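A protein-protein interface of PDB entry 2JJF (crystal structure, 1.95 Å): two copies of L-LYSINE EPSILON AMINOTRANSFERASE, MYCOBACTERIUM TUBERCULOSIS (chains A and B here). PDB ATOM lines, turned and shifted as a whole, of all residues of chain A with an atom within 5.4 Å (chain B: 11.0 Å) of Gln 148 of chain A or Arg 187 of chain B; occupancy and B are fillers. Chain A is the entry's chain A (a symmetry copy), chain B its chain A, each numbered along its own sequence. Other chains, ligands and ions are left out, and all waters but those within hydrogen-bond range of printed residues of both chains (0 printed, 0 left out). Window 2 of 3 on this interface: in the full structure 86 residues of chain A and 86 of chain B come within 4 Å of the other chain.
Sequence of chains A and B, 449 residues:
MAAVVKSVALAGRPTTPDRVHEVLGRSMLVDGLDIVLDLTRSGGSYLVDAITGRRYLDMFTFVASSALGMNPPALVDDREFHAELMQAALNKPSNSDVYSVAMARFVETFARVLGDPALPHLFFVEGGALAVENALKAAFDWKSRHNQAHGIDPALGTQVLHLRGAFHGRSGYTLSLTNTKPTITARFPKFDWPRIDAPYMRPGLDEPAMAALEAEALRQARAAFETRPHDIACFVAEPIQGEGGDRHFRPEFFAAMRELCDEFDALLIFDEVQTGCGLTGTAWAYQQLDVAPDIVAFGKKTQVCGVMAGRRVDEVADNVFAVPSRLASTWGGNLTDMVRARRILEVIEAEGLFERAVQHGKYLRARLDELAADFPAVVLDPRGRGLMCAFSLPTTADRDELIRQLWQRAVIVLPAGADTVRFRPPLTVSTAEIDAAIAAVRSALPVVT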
ATOM      1  N   PHE A 140      -7.955  25.886  15.546  1.00  0.00           N
ATOM      2  CA  PHE A 140      -8.016  24.502  16.042  1.00  0.00           C
ATOM      3  C   PHE A 140      -7.170  24.343  17.308  1.00  0.00           C
ATOM      4  O   PHE A 140      -7.609  23.753  18.303  1.00  0.00           O
ATOM      5  CB  PHE A 140      -7.506  23.508  14.995  1.00  0.00           C
ATOM      6  CG  PHE A 140      -8.348  23.424  13.748  1.00  0.00           C
ATOM      7  CD1 PHE A 140      -9.736  23.390  13.820  1.00  0.00           C
ATOM      8  CD2 PHE A 140      -7.739  23.321  12.498  1.00  0.00           C
ATOM      9  CE1 PHE A 140     -10.508  23.294  12.659  1.00  0.00           C
ATOM     10  CE2 PHE A 140      -8.503  23.222  11.330  1.00  0.00           C
ATOM     11  CZ  PHE A 140      -9.886  23.212  11.412  1.00  0.00           C
ATOM     12  N   ASP A 141      -5.950  24.867  17.250  1.00  0.00           N
ATOM     13  CA  ASP A 141      -5.044  24.846  18.388  1.00  0.00           C
ATOM     14  C   ASP A 141      -5.611  25.626  19.576  1.00  0.00           C
ATOM     15  O   ASP A 141      -5.567  25.154  20.724  1.00  0.00           O
ATOM     16  CB  ASP A 141      -3.701  25.429  17.975  1.00  0.00           C
ATOM     17  CG  ASP A 141      -2.739  25.552  19.145  1.00  0.00           C
ATOM     18  OD1 ASP A 141      -2.040  24.559  19.452  1.00  0.00           O
ATOM     19  OD2 ASP A 141      -2.681  26.651  19.736  1.00  0.00           O
ATOM     20  N   LYS A 143      -8.785  26.464  20.256  1.00  0.00           N
ATOM     21  CA  LYS A 143      -9.971  25.818  20.836  1.00  0.00           C
ATOM     22  C   LYS A 143      -9.612  24.597  21.692  1.00  0.00           C
ATOM     23  O   LYS A 143     -10.122  24.442  22.805  1.00  0.00           O
ATOM     24  CB  LYS A 143     -10.982  25.434  19.754  1.00  0.00           C
ATOM     25  CG  LYS A 143     -12.323  24.890  20.283  1.00  0.00           C
ATOM     26  CD  LYS A 143     -13.058  25.913  21.153  1.00  0.00           C
ATOM     27  CE  LYS A 143     -14.448  25.420  21.520  1.00  0.00           C
ATOM     28  NZ  LYS A 143     -15.177  26.402  22.353  1.00  0.00           N
ATOM     29  N   SER A 144      -8.739  23.741  21.169  1.00  0.00           N
ATOM     30  CA  SER A 144      -8.262  22.572  21.908  1.00  0.00           C
ATOM     31  C   SER A 144      -7.637  22.975  23.250  1.00  0.00           C
ATOM     32  O   SER A 144      -7.972  22.406  24.295  1.00  0.00           O
ATOM     33  CB  SER A 144      -7.255  21.787  21.062  1.00  0.00           C
ATOM     34  OG  SER A 144      -6.714  20.712  21.803  1.00  0.00           O
ATOM     35  N   ARG A 145      -6.750  23.969  23.212  1.00  0.00           N
ATOM     36  CA  ARG A 145      -6.065  24.458  24.408  1.00  0.00           C
ATOM     37  C   ARG A 145      -7.002  25.196  25.370  1.00  0.00           C
ATOM     38  O   ARG A 145      -6.866  25.048  26.593  1.00  0.00           O
ATOM     39  CB  ARG A 145      -4.880  25.342  24.031  1.00  0.00           C
ATOM     40  CG  ARG A 145      -3.731  24.568  23.409  1.00  0.00           C
ATOM     41  CD  ARG A 145      -2.582  25.492  23.066  1.00  0.00           C
ATOM     42  NE  ARG A 145      -1.596  24.839  22.207  1.00  0.00           N
ATOM     43  CZ  ARG A 145      -0.585  24.098  22.650  1.00  0.00           C
ATOM     44  NH1 ARG A 145       0.263  23.559  21.782  1.00  0.00           N
ATOM     45  NH2 ARG A 145      -0.417  23.888  23.957  1.00  0.00           N
ATOM     46  N   HIS A 146      -7.944  25.966  24.818  1.00  0.00           N
ATOM     47  CA  HIS A 146      -8.983  26.638  25.612  1.00  0.00           C
ATOM     48  C   HIS A 146      -9.872  25.600  26.304  1.00  0.00           C
ATOM     49  O   HIS A 146     -10.140  25.717  27.505  1.00  0.00           O
ATOM     50  CB  HIS A 146      -9.828  27.591  24.750  1.00  0.00           C
ATOM     51  CG  HIS A 146     -10.750  28.478  25.540  1.00  0.00           C
ATOM     52  ND1 HIS A 146     -12.054  28.134  25.826  1.00  0.00           N
ATOM     53  CD2 HIS A 146     -10.553  29.696  26.095  1.00  0.00           C
ATOM     54  CE1 HIS A 146     -12.621  29.101  26.526  1.00  0.00           C
ATOM     55  NE2 HIS A 146     -11.731  30.061  26.703  1.00  0.00           N
ATOM     56  N   ASN A 147     -10.311  24.591  25.548  1.00  0.00           N
ATOM     57  CA  ASN A 147     -11.049  23.453  26.102  1.00  0.00           C
ATOM     58  C   ASN A 147     -10.293  22.810  27.265  1.00  0.00           C
ATOM     59  O   ASN A 147     -10.833  22.665  28.366  1.00  0.00           O
ATOM     60  CB  ASN A 147     -11.319  22.393  25.030  1.00  0.00           C
ATOM     61  CG  ASN A 147     -12.538  22.706  24.173  1.00  0.00           C
ATOM     62  OD1 ASN A 147     -13.337  23.591  24.489  1.00  0.00           O
ATOM     63  ND2 ASN A 147     -12.692  21.957  23.083  1.00  0.00           N
ATOM     64  N   GLN A 148      -9.042  22.441  27.006  1.00  0.00           N
ATOM     65  CA  GLN A 148      -8.172  21.814  28.003  1.00  0.00           C
ATOM     66  C   GLN A 148      -8.070  22.632  29.292  1.00  0.00           C
ATOM     67  O   GLN A 148      -8.104  22.066  30.384  1.00  0.00           O
ATOM     68  CB  GLN A 148      -6.781  21.594  27.413  1.00  0.00           C
ATOM     69  CG  GLN A 148      -5.871  20.702  28.236  1.00  0.00           C
ATOM     70  CD  GLN A 148      -4.508  20.520  27.603  1.00  0.00           C
ATOM     71  OE1 GLN A 148      -4.388  20.307  26.396  1.00  0.00           O
ATOM     72  NE2 GLN A 148      -3.467  20.608  28.419  1.00  0.00           N
ATOM     73  N   ALA A 149      -7.956  23.956  29.156  1.00  0.00           N
ATOM     74  CA  ALA A 149      -7.777  24.851  30.302  1.00  0.00           C
ATOM     75  C   ALA A 149      -9.047  24.989  31.132  1.00  0.00           C
ATOM     76  O   ALA A 149      -8.990  25.427  32.281  1.00  0.00           O
ATOM     77  CB  ALA A 149      -7.286  26.229  29.843  1.00  0.00           C
ATOM     78  N   HIS A 150     -10.183  24.616  30.543  1.00  0.00           N
ATOM     79  CA  HIS A 150     -11.484  24.735  31.190  1.00  0.00           C
ATOM     80  C   HIS A 150     -12.119  23.368  31.484  1.00  0.00           C
ATOM     81  O   HIS A 150     -13.332  23.260  31.636  1.00  0.00           O
ATOM     82  CB  HIS A 150     -12.411  25.622  30.345  1.00  0.00           C
ATOM     83  CG  HIS A 150     -11.940  27.039  30.233  1.00  0.00           C
ATOM     84  ND1 HIS A 150     -12.567  28.085  30.874  1.00  0.00           N
ATOM     85  CD2 HIS A 150     -10.883  27.579  29.580  1.00  0.00           C
ATOM     86  CE1 HIS A 150     -11.926  29.210  30.611  1.00  0.00           C
ATOM     87  NE2 HIS A 150     -10.898  28.929  29.830  1.00  0.00           N
ATOM     88  N   GLY A 151     -11.289  22.333  31.562  1.00  0.00           N
ATOM     89  CA  GLY A 151     -11.735  20.999  31.958  1.00  0.00           C
ATOM     90  C   GLY A 151     -12.413  20.174  30.883  1.00  0.00           C
ATOM     91  O   GLY A 151     -12.946  19.101  31.164  1.00  0.00           O
ATOM     92  N   ILE A 152     -12.388  20.669  29.649  1.00  0.00           N
ATOM     93  CA  ILE A 152     -13.012  19.988  28.515  1.00  0.00           C
ATOM     94  C   ILE A 152     -11.962  19.186  27.731  1.00  0.00           C
ATOM     95  O   ILE A 152     -10.793  19.581  27.647  1.00  0.00           O
ATOM     96  CB  ILE A 152     -13.761  21.001  27.617  1.00  0.00           C
ATOM     97  CG1 ILE A 152     -14.857  21.706  28.431  1.00  0.00           C
ATOM     98  CG2 ILE A 152     -14.364  20.323  26.395  1.00  0.00           C
ATOM     99  CD1 ILE A 152     -15.203  23.101  27.955  1.00  0.00           C
ATOM    100  N   ASP A 153     -12.387  18.046  27.193  1.00  0.00           N
ATOM    101  CA  ASP A 153     -11.546  17.159  26.396  1.00  0.00           C
ATOM    102  C   ASP A 153     -10.831  17.937  25.270  1.00  0.00           C
ATOM    103  O   ASP A 153     -11.498  18.542  24.426  1.00  0.00           O
ATOM    104  CB  ASP A 153     -12.429  16.038  25.831  1.00  0.00           C
ATOM    105  CG  ASP A 153     -11.659  15.009  25.013  1.00  0.00           C
ATOM    106  OD1 ASP A 153     -10.407  15.025  24.990  1.00  0.00           O
ATOM    107  OD2 ASP A 153     -12.333  14.161  24.384  1.00  0.00           O
ATOM    108  N   PRO A 154      -9.479  17.949  25.281  1.00  0.00           N
ATOM    109  CA  PRO A 154      -8.687  18.652  24.255  1.00  0.00           C
ATOM    110  C   PRO A 154      -8.760  18.034  22.852  1.00  0.00           C
ATOM    111  O   PRO A 154      -8.258  18.626  21.894  1.00  0.00           O
ATOM    112  CB  PRO A 154      -7.257  18.586  24.803  1.00  0.00           C
ATOM    113  CG  PRO A 154      -7.243  17.395  25.696  1.00  0.00           C
ATOM    114  CD  PRO A 154      -8.615  17.331  26.306  1.00  0.00           C
ATOM    115  N   GLY A 157     -12.699  20.399  19.329  1.00  0.00           N
ATOM    116  CA  GLY A 157     -12.365  21.704  18.749  1.00  0.00           C
ATOM    117  C   GLY A 157     -11.806  21.594  17.339  1.00  0.00           C
ATOM    118  O   GLY A 157     -10.792  22.210  17.018  1.00  0.00           O
ATOM    119  N   ARG A 326       4.874  25.526  15.268  1.00  0.00           N
ATOM    120  CA  ARG A 326       3.477  25.090  15.111  1.00  0.00           C
ATOM    121  C   ARG A 326       2.937  25.435  13.720  1.00  0.00           C
ATOM    122  O   ARG A 326       2.212  24.641  13.115  1.00  0.00           O
ATOM    123  CB  ARG A 326       2.582  25.699  16.198  1.00  0.00           C
ATOM    124  CG  ARG A 326       2.924  25.245  17.612  1.00  0.00           C
ATOM    125  CD  ARG A 326       2.493  23.813  17.848  1.00  0.00           C
ATOM    126  NE  ARG A 326       1.045  23.701  18.007  1.00  0.00           N
ATOM    127  CZ  ARG A 326       0.310  22.699  17.528  1.00  0.00           C
ATOM    128  NH1 ARG A 326       0.879  21.720  16.829  1.00  0.00           N
ATOM    129  NH2 ARG A 326      -1.004  22.682  17.737  1.00  0.00           N
ATOM    130  N   ARG B 170       2.732  20.724   5.712  1.00  0.00           N
ATOM    131  CA  ARG B 170       1.961  21.173   6.867  1.00  0.00           C
ATOM    132  C   ARG B 170       0.583  21.716   6.474  1.00  0.00           C
ATOM    133  O   ARG B 170      -0.018  22.512   7.206  1.00  0.00           O
ATOM    134  CB  ARG B 170       2.741  22.269   7.601  1.00  0.00           C
ATOM    135  CG  ARG B 170       4.062  21.826   8.237  1.00  0.00           C
ATOM    136  CD  ARG B 170       4.786  23.081   8.728  1.00  0.00           C
ATOM    137  NE  ARG B 170       6.022  22.825   9.454  1.00  0.00           N
ATOM    138  CZ  ARG B 170       6.128  22.844  10.784  1.00  0.00           C
ATOM    139  NH1 ARG B 170       5.065  23.078  11.551  1.00  0.00           N
ATOM    140  NH2 ARG B 170       7.307  22.629  11.350  1.00  0.00           N
ATOM    141  N   GLY B 172      -3.545  21.070   4.786  1.00  0.00           N
ATOM    142  CA  GLY B 172      -4.711  20.270   5.180  1.00  0.00           C
ATOM    143  C   GLY B 172      -4.616  18.773   4.939  1.00  0.00           C
ATOM    144  O   GLY B 172      -4.895  17.990   5.843  1.00  0.00           O
ATOM    145  N   LEU B 175      -0.925  17.190   6.526  1.00  0.00           N
ATOM    146  CA  LEU B 175      -0.933  16.989   7.982  1.00  0.00           C
ATOM    147  C   LEU B 175      -1.402  15.589   8.369  1.00  0.00           C
ATOM    148  O   LEU B 175      -1.092  15.109   9.459  1.00  0.00           O
ATOM    149  CB  LEU B 175      -1.830  18.036   8.655  1.00  0.00           C
ATOM    150  CG  LEU B 175      -1.307  19.267   9.414  1.00  0.00           C
ATOM    151  CD1 LEU B 175       0.209  19.500   9.414  1.00  0.00           C
ATOM    152  CD2 LEU B 175      -2.085  20.526   9.030  1.00  0.00           C
ATOM    153  N   SER B 176      -2.157  14.945   7.481  1.00  0.00           N
ATOM    154  CA  SER B 176      -2.604  13.562   7.688  1.00  0.00           C
ATOM    155  C   SER B 176      -1.546  12.530   7.274  1.00  0.00           C
ATOM    156  O   SER B 176      -1.709  11.329   7.504  1.00  0.00           O
ATOM    157  CB  SER B 176      -3.914  13.303   6.936  1.00  0.00           C
ATOM    158  OG  SER B 176      -4.974  14.057   7.501  1.00  0.00           O
ATOM    159  N   THR B 178       2.244  13.558   7.200  1.00  0.00           N
ATOM    160  CA  THR B 178       3.444  13.917   7.950  1.00  0.00           C
ATOM    161  C   THR B 178       3.401  13.333   9.363  1.00  0.00           C
ATOM    162  O   THR B 178       2.432  13.513  10.093  1.00  0.00           O
ATOM    163  CB  THR B 178       3.602  15.455   8.003  1.00  0.00           C
ATOM    164  OG1 THR B 178       3.811  15.942   6.674  1.00  0.00           O
ATOM    165  CG2 THR B 178       4.783  15.876   8.886  1.00  0.00           C
ATOM    166  N   LYS B 181       7.830  15.032  14.062  1.00  0.00           N
ATOM    167  CA  LYS B 181       7.688  15.644  15.386  1.00  0.00           C
ATOM    168  C   LYS B 181       6.214  15.927  15.691  1.00  0.00           C
ATOM    169  O   LYS B 181       5.499  16.469  14.840  1.00  0.00           O
ATOM    170  CB  LYS B 181       8.478  16.955  15.468  1.00  0.00           C
ATOM    171  CG  LYS B 181       9.979  16.825  15.237  1.00  0.00           C
ATOM    172  CD  LYS B 181      10.649  18.202  15.266  1.00  0.00           C
ATOM    173  CE  LYS B 181      12.113  18.134  14.826  1.00  0.00           C
ATOM    174  NZ  LYS B 181      12.963  17.312  15.746  1.00  0.00           N
ATOM    175  N   PRO B 182       5.756  15.585  16.913  1.00  0.00           N
ATOM    176  CA  PRO B 182       4.360  15.819  17.318  1.00  0.00           C
ATOM    177  C   PRO B 182       3.936  17.285  17.194  1.00  0.00           C
ATOM    178  O   PRO B 182       2.772  17.564  16.917  1.00  0.00           O
ATOM    179  CB  PRO B 182       4.346  15.387  18.791  1.00  0.00           C
ATOM    180  CG  PRO B 182       5.463  14.409  18.902  1.00  0.00           C
ATOM    181  CD  PRO B 182       6.535  14.956  17.996  1.00  0.00           C
ATOM    182  N   THR B 183       4.889  18.196  17.398  1.00  0.00           N
ATOM    183  CA  THR B 183       4.683  19.646  17.289  1.00  0.00           C
ATOM    184  C   THR B 183       4.073  20.071  15.946  1.00  0.00           C
ATOM    185  O   THR B 183       3.306  21.038  15.884  1.00  0.00           O
ATOM    186  CB  THR B 183       6.024  20.392  17.498  1.00  0.00           C
ATOM    187  OG1 THR B 183       6.539  20.057  18.789  1.00  0.00           O
ATOM    188  CG2 THR B 183       5.849  21.912  17.424  1.00  0.00           C
ATOM    189  N   ILE B 184       4.422  19.353  14.882  1.00  0.00           N
ATOM    190  CA  ILE B 184       3.934  19.681  13.541  1.00  0.00           C
ATOM    191  C   ILE B 184       2.433  19.407  13.361  1.00  0.00           C
ATOM    192  O   ILE B 184       1.742  20.162  12.674  1.00  0.00           O
ATOM    193  CB  ILE B 184       4.756  18.950  12.441  1.00  0.00           C
ATOM    194  CG1 ILE B 184       6.235  19.338  12.542  1.00  0.00           C
ATOM    195  CG2 ILE B 184       4.204  19.273  11.040  1.00  0.00           C
ATOM    196  CD1 ILE B 184       7.174  18.542  11.600  1.00  0.00           C
ATOM    197  N   THR B 185       1.934  18.341  13.990  1.00  0.00           N
ATOM    198  CA  THR B 185       0.584  17.848  13.699  1.00  0.00           C
ATOM    199  C   THR B 185      -0.410  17.879  14.866  1.00  0.00           C
ATOM    200  O   THR B 185      -1.610  17.709  14.653  1.00  0.00           O
ATOM    201  CB  THR B 185       0.620  16.396  13.153  1.00  0.00           C
ATOM    202  OG1 THR B 185       1.324  15.570  14.079  1.00  0.00           O
ATOM    203  CG2 THR B 185       1.303  16.327  11.794  1.00  0.00           C
ATOM    204  N   ALA B 186       0.077  18.084  16.088  1.00  0.00           N
ATOM    205  CA  ALA B 186      -0.791  18.001  17.272  1.00  0.00           C
ATOM    206  C   ALA B 186      -1.958  18.983  17.199  1.00  0.00           C
ATOM    207  O   ALA B 186      -1.783  20.136  16.801  1.00  0.00           O
ATOM    208  CB  ALA B 186       0.018  18.222  18.553  1.00  0.00           C
ATOM    209  N   ARG B 187      -3.148  18.505  17.566  1.00  0.00           N
ATOM    210  CA  ARG B 187      -4.349  19.345  17.712  1.00  0.00           C
ATOM    211  C   ARG B 187      -4.949  19.826  16.379  1.00  0.00           C
ATOM    212  O   ARG B 187      -5.848  20.670  16.370  1.00  0.00           O
ATOM    213  CB  ARG B 187      -4.091  20.537  18.658  1.00  0.00           C
ATOM    214  CG  ARG B 187      -3.564  20.141  20.044  1.00  0.00           C
ATOM    215  CD  ARG B 187      -3.376  21.351  20.947  1.00  0.00           C
ATOM    216  NE  ARG B 187      -2.618  21.013  22.158  1.00  0.00           N
ATOM    217  CZ  ARG B 187      -3.141  20.855  23.375  1.00  0.00           C
ATOM    218  NH1 ARG B 187      -4.445  20.993  23.590  1.00  0.00           N
ATOM    219  NH2 ARG B 187      -2.343  20.558  24.393  1.00  0.00           N
ATOM    220  N   PHE B 188      -4.455  19.290  15.262  1.00  0.00           N
ATOM    221  CA  PHE B 188      -5.035  19.577  13.938  1.00  0.00           C
ATOM    222  C   PHE B 188      -5.829  18.365  13.424  1.00  0.00           C
ATOM    223  O   PHE B 188      -5.344  17.237  13.507  1.00  0.00           O
ATOM    224  CB  PHE B 188      -3.946  19.982  12.939  1.00  0.00           C
ATOM    225  CG  PHE B 188      -3.058  21.111  13.419  1.00  0.00           C
ATOM    226  CD1 PHE B 188      -3.613  22.304  13.912  1.00  0.00           C
ATOM    227  CD2 PHE B 188      -1.675  20.989  13.375  1.00  0.00           C
ATOM    228  CE1 PHE B 188      -2.792  23.345  14.358  1.00  0.00           C
ATOM    229  CE2 PHE B 188      -0.848  22.027  13.808  1.00  0.00           C
ATOM    230  CZ  PHE B 188      -1.407  23.209  14.299  1.00  0.00           C
ATOM    231  N   PRO B 189      -7.060  18.588  12.922  1.00  0.00           N
ATOM    232  CA  PRO B 189      -7.866  17.469  12.419  1.00  0.00           C
ATOM    233  C   PRO B 189      -7.212  16.709  11.252  1.00  0.00           C
ATOM    234  O   PRO B 189      -6.572  17.306  10.374  1.00  0.00           O
ATOM    235  CB  PRO B 189      -9.191  18.125  11.990  1.00  0.00           C
ATOM    236  CG  PRO B 189      -8.930  19.584  11.938  1.00  0.00           C
ATOM    237  CD  PRO B 189      -7.774  19.874  12.842  1.00  0.00           C
ATOM    238  N   LYS B 190      -7.374  15.395  11.272  1.00  0.00           N
ATOM    239  CA  LYS B 190      -6.701  14.518  10.321  1.00  0.00           C
ATOM    240  C   LYS B 190      -7.677  13.487   9.782  1.00  0.00           C
ATOM    241  O   LYS B 190      -8.698  13.201  10.415  1.00  0.00           O
ATOM    242  CB  LYS B 190      -5.511  13.819  10.993  1.00  0.00           C
ATOM    243  CG  LYS B 190      -4.339  14.747  11.307  1.00  0.00           C
ATOM    244  CD  LYS B 190      -3.215  14.040  12.071  1.00  0.00           C
ATOM    245  CE  LYS B 190      -3.425  14.077  13.579  1.00  0.00           C
ATOM    246  NZ  LYS B 190      -3.319  15.461  14.145  1.00  0.00           N
ATOM    247  N   PHE B 191      -7.376  12.958   8.599  1.00  0.00           N
ATOM    248  CA  PHE B 191      -8.071  11.793   8.078  1.00  0.00           C
ATOM    249  C   PHE B 191      -7.377  10.572   8.639  1.00  0.00           C
ATOM    250  O   PHE B 191      -6.175  10.599   8.911  1.00  0.00           O
ATOM    251  CB  PHE B 191      -8.007  11.745   6.547  1.00  0.00           C
ATOM    252  CG  PHE B 191      -8.743  12.868   5.865  1.00  0.00           C
ATOM    253  CD1 PHE B 191     -10.105  12.773   5.612  1.00  0.00           C
ATOM    254  CD2 PHE B 191      -8.072  14.018   5.472  1.00  0.00           C
ATOM    255  CE1 PHE B 191     -10.795  13.814   4.984  1.00  0.00           C
ATOM    256  CE2 PHE B 191      -8.755  15.064   4.840  1.00  0.00           C
ATOM    257  CZ  PHE B 191     -10.115  14.956   4.597  1.00  0.00           C
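No position is printed for both chains. Of the 12 pairs that touch across the chains among the printed residues, none has its exchanged pair printed and touching as well.
Printed residues of chain B within 4 Å of Gln 148 of chain A: Arg 187 (2.9 Å). Printed residues of chain A within 4 Å of Arg 187 of chain B: Phe 140, Asp 141, Ser 144, Arg 145, Gln 148, Pro 154 and Arg 326. Phe 140 of chain A touches two residues of chain B. No residue of chain B comes within 4 Å of Asn 147 of chain A. No residue of chain B comes within 4 Å of Ala 149 of chain A. No residue of chain B comes within 4 Å of Gly 151 of chain A. No residue of chain B comes within 4 Å of Ile 152 of chain A. Pro 154 of chain A touches one residue of chain B. Of the printed residues of chain A, Pro 189 of chain B touches Phe 140 (3.5 Å). Printed residues of chain A within 4 Å of Thr 183 of chain B: Arg 326. Of the printed residues of chain B, Arg 326 of chain A touches Arg 170 (3.6 Å), Thr 183 (2.7 Å), Ala 186 (2.8 Å), Arg 187 (3.9 Å) and Phe 188 (3.5 Å). Of the printed residues of chain A, Ala 186 of chain B touches Arg 326. Ile 184 of chain B touches none of the printed residues of chain A. The nearest residue of chain B that does not touch Gln 148 of chain A is Ala 186 of chain B (9.2 Å). The nearest printed residue of chain A that does not touch Phe 188 of chain B is Phe 140 of chain A (4.2 Å).
The side-chain amino group (NZ) of Lys 190 of chain B sits at hydrogen-bond distance from the backbone carbonyl oxygen (O) of Phe 188 of chain B, at 2.8 Å. The side-chain carboxylate of Asp 141 of chain A is in salt-bridge range of the guanidinium group of Arg 145 of chain A (2.8 Å). OD1 of Asp 141 of chain A is in salt-bridge range of NH2 of Arg 326 of chain A (2.7 Å). The backbone carbonyl oxygen (O) of Pro 154 of chain A sits at hydrogen-bond distance from the side-chain hydroxyl (OG) of Ser 144 of chain A (2.6 Å).
Among the printed residues, pairs that only touch across the chains: Phe 140 of chain A with Pro 189 of chain B (3.5 Å), Arg 326 of chain A with Phe 188 of chain B (3.5 Å), Phe 140 of chain A with Arg 187 of chain B (3.6 Å), Arg 326 of chain A with Arg 170 of chain B (3.6 Å), Arg 145 of chain A with Arg 187 of chain B (3.7 Å), Asp 141 of chain A with Arg 187 of chain B (3.8 Å), Arg 326 of chain A with Arg 187 of chain B (3.9 Å) and Pro 154 of chain A with Arg 187 of chain B (3.9 Å).
Of the 16 printed residues of chain B, 6 touch a printed residue of chain A. Hydrophobic or aromatic side chains of chain B that line the printed part of chain A: Ala 186, Phe 188 and Pro 189. Along chain B the printed residues that touch a printed residue of chain A span positions 170 to 189. Of the 16 printed residues of chain A, 7 touch a printed residue of chain B. Printed residues of chain A that touch a printed residue of chain B: Phe 140, Asp 141, Ser 144, Arg 145, Gln 148, Pro 154 and Arg 326. Along chain A the printed residues that touch a printed residue of chain B span positions 140 to 326. Among the printed residues, 12 pairs touch across the chains.
NH1 of Arg 326 of chain A sits at hydrogen-bond distance from O of Thr 183 of chain B, at 2.7 Å. NH2 of Arg 326 of chain A lies within hydrogen-bond range of O of Ala 186 of chain B, at 2.8 Å. The guanidinium group (NH1) of Arg 187 of chain B sits at hydrogen-bond distance from the side-chain hydroxyl (OG) of Ser 144 of chain A. The guanidinium group (NH2) of Arg 187 of chain B lies within hydrogen-bond range of the side-chain amide oxygen (OE1) of Gln 148 of chain A (2.9 Å).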
